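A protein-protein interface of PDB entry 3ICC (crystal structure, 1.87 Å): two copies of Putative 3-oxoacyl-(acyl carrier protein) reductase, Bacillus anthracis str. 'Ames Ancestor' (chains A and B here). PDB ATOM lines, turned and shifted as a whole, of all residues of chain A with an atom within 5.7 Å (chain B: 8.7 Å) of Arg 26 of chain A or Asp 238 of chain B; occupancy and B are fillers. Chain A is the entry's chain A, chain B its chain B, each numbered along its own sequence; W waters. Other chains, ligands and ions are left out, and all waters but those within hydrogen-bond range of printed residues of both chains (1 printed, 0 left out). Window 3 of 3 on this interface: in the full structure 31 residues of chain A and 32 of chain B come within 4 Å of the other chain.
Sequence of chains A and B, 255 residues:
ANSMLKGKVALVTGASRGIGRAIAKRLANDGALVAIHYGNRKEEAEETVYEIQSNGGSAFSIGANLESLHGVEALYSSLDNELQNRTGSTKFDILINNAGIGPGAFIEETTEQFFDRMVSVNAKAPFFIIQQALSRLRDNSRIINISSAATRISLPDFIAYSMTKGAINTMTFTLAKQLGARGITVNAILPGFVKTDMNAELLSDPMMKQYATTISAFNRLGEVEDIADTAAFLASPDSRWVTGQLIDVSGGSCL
The side-chain carboxylate (OD2) of Asp 238 of chain B lies within salt-bridge range of the guanidinium group (NH2) of Arg 26 of chain A (2.9 Å). The side-chain carboxylate (OD1) of Asp 226 of chain A lies within salt-bridge range of the guanidinium group (NH2) of Arg 240 of chain B, at 3.3 Å. The side-chain carboxylate of Asp 229 of chain A lies within salt-bridge range of the guanidinium group of Arg 240 of chain B (3.1 Å).
NE of Arg 26 of chain A is in salt-bridge range of OD2 of Asp 30 of chain A (2.9 Å). The guanidinium group of Arg 26 of chain A lies within salt-bridge range of the side-chain carboxylate of Asp 229 of chain A (2.7 Å). The backbone carbonyl oxygen (O) of Phe 233 of chain B lies within hydrogen-bond range of the side-chain hydroxyl (OG) of Ser 236 of chain B (2.8 Å). The backbone carbonyl oxygen (O) of Phe 233 of chain B sits at hydrogen-bond distance from the side-chain hydroxyl (OG) of Ser 239 of chain B, 3.0 Å away. N of Asp 238 of chain B sits close to OG of Ser 236 of chain B (3.3 Å). NH1 of Arg 240 of chain B lies within hydrogen-bond range of O of Pro 237 of chain B (3.3 Å).
Asp 226 of chain A touches Trp 241 of chain B. Asp 229 of chain A touches Phe 233 of chain B. CB of Asp 229 of chain A touches O of Asp 238 of chain B, 3.4 Å away. Thr 230 of chain A touches Phe 233 of chain B. Val 242 of chain B touches Thr 230 of chain A (CG2 to OG1, 3.4 Å).
Lys 25 of chain A touches none of the printed residues of chain B. Asn 29 of chain A touches none of the printed residues of chain B. Of the printed residues of chain B, Asp 229 of chain A touches Phe 233 (3.8 Å), Asp 238 (3.4 Å) and Arg 240 (3.1 Å). Printed residues of chain B within 4 Å of Thr 230 of chain A: Phe 233 (3.5 Å) and Val 242 (3.4 Å). Of chain A, only Arg 26 and Asp 229 come within 4 Å of Asp 238 of chain B. Of the printed residues of chain A, Arg 240 of chain B touches Asp 226 (3.3 Å) and Asp 229 (3.1 Å). Of the printed residues of chain A, Trp 241 of chain B touches Asp 226 (3.6 Å). The nearest residue of chain B that does not touch Arg 26 of chain A is Met 4 of chain B (6.0 Å).
Printed residues of chain A that touch a printed residue of chain B: Arg 26, Asp 226, Asp 229 and Thr 230. Along chain A the printed residues that touch a printed residue of chain B span positions 26 to 230. Of the 15 printed residues of chain B, 5 touch a printed residue of chain A. Printed residues of chain B that touch a printed residue of chain A: Phe 233, Asp 238, Arg 240, Trp 241 and Val 242. Hydrophobic or aromatic side chains of chain B within 4 Å of the printed part of chain A: Phe 233, Trp 241 and Val 242. Among the printed residues, 8 pairs touch across the chains.
Positions printed for both chains: 5 and 232. Of the 8 pairs that touch across the chains among the printed residues, none has its exchanged pair printed and touching as well.
Water W1 lies within hydrogen-bond range of O of Asp 238 of chain B, O of Asp 226 of chain A, N of Trp 241 of chain B and OG1 of Thr 230 of chain A.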
ATOM      1  N   ASN A   2      21.821  26.725 -23.447  1.00  0.00           N
ATOM      2  CA  ASN A   2      22.984  27.277 -22.764  1.00  0.00           C
ATOM      3  C   ASN A   2      23.921  27.985 -23.752  1.00  0.00           C
ATOM      4  O   ASN A   2      24.208  27.446 -24.829  1.00  0.00           O
ATOM      5  CB  ASN A   2      23.739  26.159 -22.018  1.00  0.00           C
ATOM      6  CG  ASN A   2      24.756  26.695 -21.025  1.00  0.00           C
ATOM      7  OD1 ASN A   2      25.668  27.434 -21.399  1.00  0.00           O
ATOM      8  ND2 ASN A   2      24.623  26.295 -19.748  1.00  0.00           N
ATOM      9  N   LEU A   5      29.324  29.674 -22.367  1.00  0.00           N
ATOM     10  CA  LEU A   5      30.726  29.753 -22.781  1.00  0.00           C
ATOM     11  C   LEU A   5      30.897  30.430 -24.158  1.00  0.00           C
ATOM     12  O   LEU A   5      31.939  30.315 -24.819  1.00  0.00           O
ATOM     13  CB  LEU A   5      31.341  28.344 -22.751  1.00  0.00           C
ATOM     14  CG  LEU A   5      31.201  27.567 -21.441  1.00  0.00           C
ATOM     15  CD1 LEU A   5      31.941  26.207 -21.584  1.00  0.00           C
ATOM     16  CD2 LEU A   5      31.796  28.377 -20.237  1.00  0.00           C
ATOM     17  N   ARG A  21      35.871  13.060 -24.270  1.00  0.00           N
ATOM     18  CA  ARG A  21      34.940  13.291 -25.322  1.00  0.00           C
ATOM     19  C   ARG A  21      33.631  13.934 -24.797  1.00  0.00           C
ATOM     20  O   ARG A  21      33.034  14.812 -25.443  1.00  0.00           O
ATOM     21  CB  ARG A  21      34.622  11.981 -26.056  1.00  0.00           C
ATOM     22  CG  ARG A  21      33.503  12.185 -27.058  1.00  0.00           C
ATOM     23  CD  ARG A  21      32.754  10.962 -27.375  1.00  0.00           C
ATOM     24  NE  ARG A  21      33.519  10.034 -28.143  1.00  0.00           N
ATOM     25  CZ  ARG A  21      33.489   8.696 -28.005  1.00  0.00           C
ATOM     26  NH1 ARG A  21      32.785   8.106 -27.037  1.00  0.00           N
ATOM     27  NH2 ARG A  21      34.220   7.935 -28.828  1.00  0.00           N
ATOM     28  N   ALA A  22      33.176  13.496 -23.634  1.00  0.00           N
ATOM     29  CA  ALA A  22      31.929  14.023 -23.074  1.00  0.00           C
ATOM     30  C   ALA A  22      32.074  15.458 -22.662  1.00  0.00           C
ATOM     31  O   ALA A  22      31.129  16.224 -22.865  1.00  0.00           O
ATOM     32  CB  ALA A  22      31.335  13.120 -21.921  1.00  0.00           C
ATOM     33  N   ILE A  23      33.234  15.810 -22.075  1.00  0.00           N
ATOM     34  CA  ILE A  23      33.544  17.188 -21.677  1.00  0.00           C
ATOM     35  C   ILE A  23      33.585  18.047 -22.934  1.00  0.00           C
ATOM     36  O   ILE A  23      33.019  19.116 -22.935  1.00  0.00           O
ATOM     37  CB  ILE A  23      34.881  17.307 -20.870  1.00  0.00           C
ATOM     38  CG1 ILE A  23      34.720  16.564 -19.524  1.00  0.00           C
ATOM     39  CG2 ILE A  23      35.309  18.828 -20.660  1.00  0.00           C
ATOM     40  CD1 ILE A  23      35.985  16.262 -18.695  1.00  0.00           C
ATOM     41  N   ALA A  24      34.292  17.602 -23.974  1.00  0.00           N
ATOM     42  CA  ALA A  24      34.320  18.324 -25.240  1.00  0.00           C
ATOM     43  C   ALA A  24      32.923  18.586 -25.820  1.00  0.00           C
ATOM     44  O   ALA A  24      32.603  19.735 -26.186  1.00  0.00           O
ATOM     45  CB  ALA A  24      35.243  17.630 -26.262  1.00  0.00           C
ATOM     46  N   LYS A  25      32.062  17.579 -25.845  1.00  0.00           N
ATOM     47  CA  LYS A  25      30.686  17.781 -26.343  1.00  0.00           C
ATOM     48  C   LYS A  25      29.917  18.814 -25.515  1.00  0.00           C
ATOM     49  O   LYS A  25      29.225  19.658 -26.064  1.00  0.00           O
ATOM     50  CB  LYS A  25      29.915  16.451 -26.417  1.00  0.00           C
ATOM     51  CG  LYS A  25      30.514  15.540 -27.491  1.00  0.00           C
ATOM     52  CD  LYS A  25      29.585  14.491 -28.034  1.00  0.00           C
ATOM     53  CE  LYS A  25      29.081  13.535 -27.035  1.00  0.00           C
ATOM     54  NZ  LYS A  25      28.690  12.225 -27.713  1.00  0.00           N
ATOM     55  N   ARG A  26      30.038  18.731 -24.198  1.00  0.00           N
ATOM     56  CA  ARG A  26      29.307  19.596 -23.302  1.00  0.00           C
ATOM     57  C   ARG A  26      29.789  21.028 -23.427  1.00  0.00           C
ATOM     58  O   ARG A  26      28.938  21.952 -23.490  1.00  0.00           O
ATOM     59  CB  ARG A  26      29.471  19.177 -21.848  1.00  0.00           C
ATOM     60  CG  ARG A  26      28.828  20.111 -20.819  1.00  0.00           C
ATOM     61  CD  ARG A  26      27.340  20.328 -21.021  1.00  0.00           C
ATOM     62  NE  ARG A  26      26.941  21.537 -20.287  1.00  0.00           N
ATOM     63  CZ  ARG A  26      26.223  21.546 -19.171  1.00  0.00           C
ATOM     64  NH1 ARG A  26      25.813  20.412 -18.637  1.00  0.00           N
ATOM     65  NH2 ARG A  26      25.923  22.698 -18.592  1.00  0.00           N
ATOM     66  N   LEU A  27      31.120  21.217 -23.400  1.00  0.00           N
ATOM     67  CA  LEU A  27      31.679  22.580 -23.551  1.00  0.00           C
ATOM     68  C   LEU A  27      31.253  23.248 -24.864  1.00  0.00           C
ATOM     69  O   LEU A  27      30.869  24.430 -24.858  1.00  0.00           O
ATOM     70  CB  LEU A  27      33.203  22.566 -23.445  1.00  0.00           C
ATOM     71  CG  LEU A  27      33.747  22.124 -22.073  1.00  0.00           C
ATOM     72  CD1 LEU A  27      35.301  22.083 -22.120  1.00  0.00           C
ATOM     73  CD2 LEU A  27      33.243  23.051 -20.958  1.00  0.00           C
ATOM     74  N   ALA A  28      31.295  22.488 -25.962  1.00  0.00           N
ATOM     75  CA  ALA A  28      30.825  22.962 -27.273  1.00  0.00           C
ATOM     76  C   ALA A  28      29.340  23.273 -27.295  1.00  0.00           C
ATOM     77  O   ALA A  28      28.928  24.246 -27.939  1.00  0.00           O
ATOM     78  CB  ALA A  28      31.175  21.937 -28.379  1.00  0.00           C
ATOM     79  N   ASN A  29      28.537  22.462 -26.587  1.00  0.00           N
ATOM     80  CA  ASN A  29      27.092  22.705 -26.444  1.00  0.00           C
ATOM     81  C   ASN A  29      26.837  24.036 -25.752  1.00  0.00           C
ATOM     82  O   ASN A  29      25.862  24.708 -26.080  1.00  0.00           O
ATOM     83  CB  ASN A  29      26.394  21.564 -25.655  1.00  0.00           C
ATOM     84  CG  ASN A  29      24.877  21.782 -25.508  1.00  0.00           C
ATOM     85  OD1 ASN A  29      24.092  21.350 -26.362  1.00  0.00           O
ATOM     86  ND2 ASN A  29      24.472  22.499 -24.449  1.00  0.00           N
ATOM     87  N   ASP A  30      27.739  24.444 -24.852  1.00  0.00           N
ATOM     88  CA  ASP A  30      27.589  25.678 -24.086  1.00  0.00           C
ATOM     89  C   ASP A  30      28.176  26.905 -24.806  1.00  0.00           C
ATOM     90  O   ASP A  30      28.131  28.003 -24.272  1.00  0.00           O
ATOM     91  CB  ASP A  30      28.212  25.539 -22.675  1.00  0.00           C
ATOM     92  CG  ASP A  30      27.426  24.573 -21.759  1.00  0.00           C
ATOM     93  OD1 ASP A  30      26.309  24.166 -22.113  1.00  0.00           O
ATOM     94  OD2 ASP A  30      27.937  24.231 -20.685  1.00  0.00           O
ATOM     95  N   GLY A  31      28.676  26.715 -26.021  1.00  0.00           N
ATOM     96  CA  GLY A  31      29.118  27.806 -26.880  1.00  0.00           C
ATOM     97  C   GLY A  31      30.626  27.918 -27.119  1.00  0.00           C
ATOM     98  O   GLY A  31      31.048  28.708 -27.947  1.00  0.00           O
ATOM     99  N   ASP A 226      27.997  12.660 -16.287  1.00  0.00           N
ATOM    100  CA  ASP A 226      28.040  13.101 -14.896  1.00  0.00           C
ATOM    101  C   ASP A 226      29.289  13.933 -14.637  1.00  0.00           C
ATOM    102  O   ASP A 226      29.240  14.881 -13.856  1.00  0.00           O
ATOM    103  CB  ASP A 226      28.057  11.939 -13.917  1.00  0.00           C
ATOM    104  CG  ASP A 226      26.760  11.124 -13.943  1.00  0.00           C
ATOM    105  OD1 ASP A 226      25.673  11.722 -13.784  1.00  0.00           O
ATOM    106  OD2 ASP A 226      26.810   9.894 -14.131  1.00  0.00           O
ATOM    107  N   ALA A 228      31.146  15.416 -17.173  1.00  0.00           N
ATOM    108  CA  ALA A 228      31.132  16.548 -18.093  1.00  0.00           C
ATOM    109  C   ALA A 228      30.280  17.649 -17.538  1.00  0.00           C
ATOM    110  O   ALA A 228      30.628  18.807 -17.703  1.00  0.00           O
ATOM    111  CB  ALA A 228      30.657  16.159 -19.496  1.00  0.00           C
ATOM    112  N   ASP A 229      29.166  17.291 -16.891  1.00  0.00           N
ATOM    113  CA  ASP A 229      28.274  18.319 -16.326  1.00  0.00           C
ATOM    114  C   ASP A 229      28.863  19.121 -15.167  1.00  0.00           C
ATOM    115  O   ASP A 229      28.544  20.316 -15.013  1.00  0.00           O
ATOM    116  CB  ASP A 229      26.902  17.726 -16.017  1.00  0.00           C
ATOM    117  CG  ASP A 229      26.164  17.310 -17.287  1.00  0.00           C
ATOM    118  OD1 ASP A 229      26.531  17.769 -18.397  1.00  0.00           O
ATOM    119  OD2 ASP A 229      25.248  16.475 -17.202  1.00  0.00           O
ATOM    120  N   THR A 230      29.754  18.526 -14.373  1.00  0.00           N
ATOM    121  CA  THR A 230      30.467  19.279 -13.350  1.00  0.00           C
ATOM    122  C   THR A 230      31.615  20.106 -13.958  1.00  0.00           C
ATOM    123  O   THR A 230      31.863  21.257 -13.551  1.00  0.00           O
ATOM    124  CB  THR A 230      31.007  18.342 -12.233  1.00  0.00           C
ATOM    125  OG1 THR A 230      29.892  17.840 -11.486  1.00  0.00           O
ATOM    126  CG2 THR A 230      31.922  19.061 -11.262  1.00  0.00           C
ATOM    127  N   ALA A 232      31.504  21.478 -16.742  1.00  0.00           N
ATOM    128  CA  ALA A 232      30.852  22.661 -17.368  1.00  0.00           C
ATOM    129  C   ALA A 232      30.719  23.821 -16.376  1.00  0.00           C
ATOM    130  O   ALA A 232      30.886  24.993 -16.779  1.00  0.00           O
ATOM    131  CB  ALA A 232      29.469  22.312 -17.981  1.00  0.00           C
ATOM    132  N   MET B   4      16.743  26.756 -16.542  1.00  0.00           N
ATOM    133  CA  MET B   4      17.432  25.631 -15.911  1.00  0.00           C
ATOM    134  C   MET B   4      16.585  24.982 -14.769  1.00  0.00           C
ATOM    135  O   MET B   4      16.546  23.757 -14.634  1.00  0.00           O
ATOM    136  CB  MET B   4      18.778  26.156 -15.384  1.00  0.00           C
ATOM    137  CG  MET B   4      19.685  25.158 -14.667  1.00  0.00           C
ATOM    138  SD  MET B   4      20.357  23.714 -15.844  1.00  0.00           S
ATOM    139  CE  MET B   4      20.370  24.680 -17.573  1.00  0.00           C
ATOM    140  N   LEU B   5      15.878  25.796 -13.988  1.00  0.00           N
ATOM    141  CA  LEU B   5      15.089  25.300 -12.838  1.00  0.00           C
ATOM    142  C   LEU B   5      13.576  25.464 -13.025  1.00  0.00           C
ATOM    143  O   LEU B   5      12.806  25.470 -12.044  1.00  0.00           O
ATOM    144  CB  LEU B   5      15.520  26.009 -11.549  1.00  0.00           C
ATOM    145  CG  LEU B   5      17.004  25.944 -11.154  1.00  0.00           C
ATOM    146  CD1 LEU B   5      17.236  26.690  -9.866  1.00  0.00           C
ATOM    147  CD2 LEU B   5      17.520  24.473 -11.037  1.00  0.00           C
ATOM    148  N   ARG B 142      17.531  18.665  -3.961  1.00  0.00           N
ATOM    149  CA  ARG B 142      18.809  19.241  -3.623  1.00  0.00           C
ATOM    150  C   ARG B 142      18.723  19.946  -2.278  1.00  0.00           C
ATOM    151  O   ARG B 142      17.796  20.733  -2.014  1.00  0.00           O
ATOM    152  CB  ARG B 142      19.200  20.279  -4.679  1.00  0.00           C
ATOM    153  CG  ARG B 142      19.201  19.753  -6.088  1.00  0.00           C
ATOM    154  CD  ARG B 142      20.451  18.940  -6.192  1.00  0.00           C
ATOM    155  NE  ARG B 142      20.792  18.596  -7.539  1.00  0.00           N
ATOM    156  CZ  ARG B 142      20.533  17.434  -8.117  1.00  0.00           C
ATOM    157  NH1 ARG B 142      19.894  16.470  -7.481  1.00  0.00           N
ATOM    158  NH2 ARG B 142      20.951  17.243  -9.350  1.00  0.00           N
ATOM    159  N   THR B 185      20.727  15.053  -3.396  1.00  0.00           N
ATOM    160  CA  THR B 185      22.089  15.376  -3.057  1.00  0.00           C
ATOM    161  C   THR B 185      22.053  16.321  -1.853  1.00  0.00           C
ATOM    162  O   THR B 185      21.074  17.045  -1.618  1.00  0.00           O
ATOM    163  CB  THR B 185      22.914  16.047  -4.210  1.00  0.00           C
ATOM    164  OG1 THR B 185      22.383  17.336  -4.469  1.00  0.00           O
ATOM    165  CG2 THR B 185      22.868  15.215  -5.532  1.00  0.00           C
ATOM    166  N   ALA B 232      23.688  28.012  -7.411  1.00  0.00           N
ATOM    167  CA  ALA B 232      22.899  27.697  -8.594  1.00  0.00           C
ATOM    168  C   ALA B 232      23.304  26.373  -9.246  1.00  0.00           C
ATOM    169  O   ALA B 232      22.428  25.610  -9.750  1.00  0.00           O
ATOM    170  CB  ALA B 232      22.983  28.822  -9.643  1.00  0.00           C
ATOM    171  N   PHE B 233      24.598  26.104  -9.280  1.00  0.00           N
ATOM    172  CA  PHE B 233      25.090  24.817  -9.802  1.00  0.00           C
ATOM    173  C   PHE B 233      24.640  23.659  -8.927  1.00  0.00           C
ATOM    174  O   PHE B 233      24.136  22.657  -9.430  1.00  0.00           O
ATOM    175  CB  PHE B 233      26.629  24.808  -9.904  1.00  0.00           C
ATOM    176  CG  PHE B 233      27.221  23.401 -10.112  1.00  0.00           C
ATOM    177  CD1 PHE B 233      26.996  22.712 -11.283  1.00  0.00           C
ATOM    178  CD2 PHE B 233      28.003  22.794  -9.128  1.00  0.00           C
ATOM    179  CE1 PHE B 233      27.518  21.419 -11.490  1.00  0.00           C
ATOM    180  CE2 PHE B 233      28.540  21.504  -9.338  1.00  0.00           C
ATOM    181  CZ  PHE B 233      28.269  20.818 -10.531  1.00  0.00           C
ATOM    182  N   LEU B 234      24.850  23.779  -7.623  1.00  0.00           N
ATOM    183  CA  LEU B 234      24.451  22.713  -6.691  1.00  0.00           C
ATOM    184  C   LEU B 234      22.916  22.479  -6.707  1.00  0.00           C
ATOM    185  O   LEU B 234      22.479  21.349  -6.554  1.00  0.00           O
ATOM    186  CB  LEU B 234      24.968  22.973  -5.268  1.00  0.00           C
ATOM    187  CG  LEU B 234      26.502  22.982  -5.142  1.00  0.00           C
ATOM    188  CD1 LEU B 234      26.930  23.357  -3.731  1.00  0.00           C
ATOM    189  CD2 LEU B 234      27.157  21.654  -5.494  1.00  0.00           C
ATOM    190  N   ALA B 235      22.125  23.522  -6.939  1.00  0.00           N
ATOM    191  CA  ALA B 235      20.666  23.395  -7.068  1.00  0.00           C
ATOM    192  C   ALA B 235      20.183  22.750  -8.373  1.00  0.00           C
ATOM    193  O   ALA B 235      19.007  22.356  -8.477  1.00  0.00           O
ATOM    194  CB  ALA B 235      20.001  24.767  -6.906  1.00  0.00           C
ATOM    195  N   SER B 236      21.065  22.674  -9.369  1.00  0.00           N
ATOM    196  CA  SER B 236      20.697  22.273 -10.726  1.00  0.00           C
ATOM    197  C   SER B 236      20.838  20.790 -11.006  1.00  0.00           C
ATOM    198  O   SER B 236      21.548  20.091 -10.283  1.00  0.00           O
ATOM    199  CB  SER B 236      21.530  23.035 -11.742  1.00  0.00           C
ATOM    200  OG  SER B 236      22.811  22.459 -11.900  1.00  0.00           O
ATOM    201  N   PRO B 237      20.171  20.300 -12.087  1.00  0.00           N
ATOM    202  CA  PRO B 237      20.359  18.891 -12.467  1.00  0.00           C
ATOM    203  C   PRO B 237      21.799  18.516 -12.842  1.00  0.00           C
ATOM    204  O   PRO B 237      22.195  17.384 -12.578  1.00  0.00           O
ATOM    205  CB  PRO B 237      19.387  18.706 -13.659  1.00  0.00           C
ATOM    206  CG  PRO B 237      18.289  19.722 -13.390  1.00  0.00           C
ATOM    207  CD  PRO B 237      19.080  20.925 -12.867  1.00  0.00           C
ATOM    208  N   ASP B 238      22.577  19.464 -13.358  1.00  0.00           N
ATOM    209  CA  ASP B 238      24.007  19.306 -13.680  1.00  0.00           C
ATOM    210  C   ASP B 238      24.900  18.756 -12.542  1.00  0.00           C
ATOM    211  O   ASP B 238      25.941  18.170 -12.822  1.00  0.00           O
ATOM    212  CB  ASP B 238      24.617  20.664 -14.126  1.00  0.00           C
ATOM    213  CG  ASP B 238      24.254  21.049 -15.583  1.00  0.00           C
ATOM    214  OD1 ASP B 238      23.641  20.241 -16.295  1.00  0.00           O
ATOM    215  OD2 ASP B 238      24.624  22.165 -16.020  1.00  0.00           O
ATOM    216  N   SER B 239      24.499  18.962 -11.276  1.00  0.00           N
ATOM    217  CA  SER B 239      25.301  18.568 -10.141  1.00  0.00           C
ATOM    218  C   SER B 239      24.905  17.216  -9.526  1.00  0.00           C
ATOM    219  O   SER B 239      25.282  16.906  -8.406  1.00  0.00           O
ATOM    220  CB  SER B 239      25.232  19.662  -9.066  1.00  0.00           C
ATOM    221  OG  SER B 239      23.958  19.805  -8.538  1.00  0.00           O
ATOM    222  N   ARG B 240      24.196  16.392 -10.294  1.00  0.00           N
ATOM    223  CA  ARG B 240      23.648  15.145  -9.775  1.00  0.00           C
ATOM    224  C   ARG B 240      24.684  14.173  -9.197  1.00  0.00           C
ATOM    225  O   ARG B 240      24.339  13.343  -8.357  1.00  0.00           O
ATOM    226  CB  ARG B 240      22.866  14.437 -10.868  1.00  0.00           C
ATOM    227  CG  ARG B 240      23.731  13.733 -11.895  1.00  0.00           C
ATOM    228  CD  ARG B 240      22.858  13.199 -13.073  1.00  0.00           C
ATOM    229  NE  ARG B 240      22.397  14.284 -13.931  1.00  0.00           N
ATOM    230  CZ  ARG B 240      23.194  14.954 -14.757  1.00  0.00           C
ATOM    231  NH1 ARG B 240      22.704  15.928 -15.496  1.00  0.00           N
ATOM    232  NH2 ARG B 240      24.493  14.647 -14.836  1.00  0.00           N
ATOM    233  N   TRP B 241      25.945  14.279  -9.622  1.00  0.00           N
ATOM    234  CA  TRP B 241      26.973  13.306  -9.200  1.00  0.00           C
ATOM    235  C   TRP B 241      27.886  13.862  -8.104  1.00  0.00           C
ATOM    236  O   TRP B 241      28.888  13.242  -7.751  1.00  0.00           O
ATOM    237  CB  TRP B 241      27.754  12.826 -10.441  1.00  0.00           C
ATOM    238  CG  TRP B 241      28.206  11.374 -10.384  1.00  0.00           C
ATOM    239  CD1 TRP B 241      29.475  10.895 -10.616  1.00  0.00           C
ATOM    240  CD2 TRP B 241      27.408  10.242 -10.065  1.00  0.00           C
ATOM    241  NE1 TRP B 241      29.510   9.538 -10.466  1.00  0.00           N
ATOM    242  CE2 TRP B 241      28.251   9.104 -10.129  1.00  0.00           C
ATOM    243  CE3 TRP B 241      26.057  10.062  -9.743  1.00  0.00           C
ATOM    244  CZ2 TRP B 241      27.792   7.823  -9.869  1.00  0.00           C
ATOM    245  CZ3 TRP B 241      25.591   8.754  -9.503  1.00  0.00           C
ATOM    246  CH2 TRP B 241      26.456   7.671  -9.550  1.00  0.00           C
ATOM    247  N   VAL B 242      27.553  15.063  -7.610  1.00  0.00           N
ATOM    248  CA  VAL B 242      28.265  15.703  -6.524  1.00  0.00           C
ATOM    249  C   VAL B 242      27.345  15.671  -5.312  1.00  0.00           C
ATOM    250  O   VAL B 242      26.277  16.324  -5.289  1.00  0.00           O
ATOM    251  CB  VAL B 242      28.608  17.174  -6.866  1.00  0.00           C
ATOM    252  CG1 VAL B 242      29.337  17.867  -5.723  1.00  0.00           C
ATOM    253  CG2 VAL B 242      29.447  17.231  -8.155  1.00  0.00           C
HETATM  254  O   HOH W   1      27.320  15.961 -11.892  1.00  0.00           O
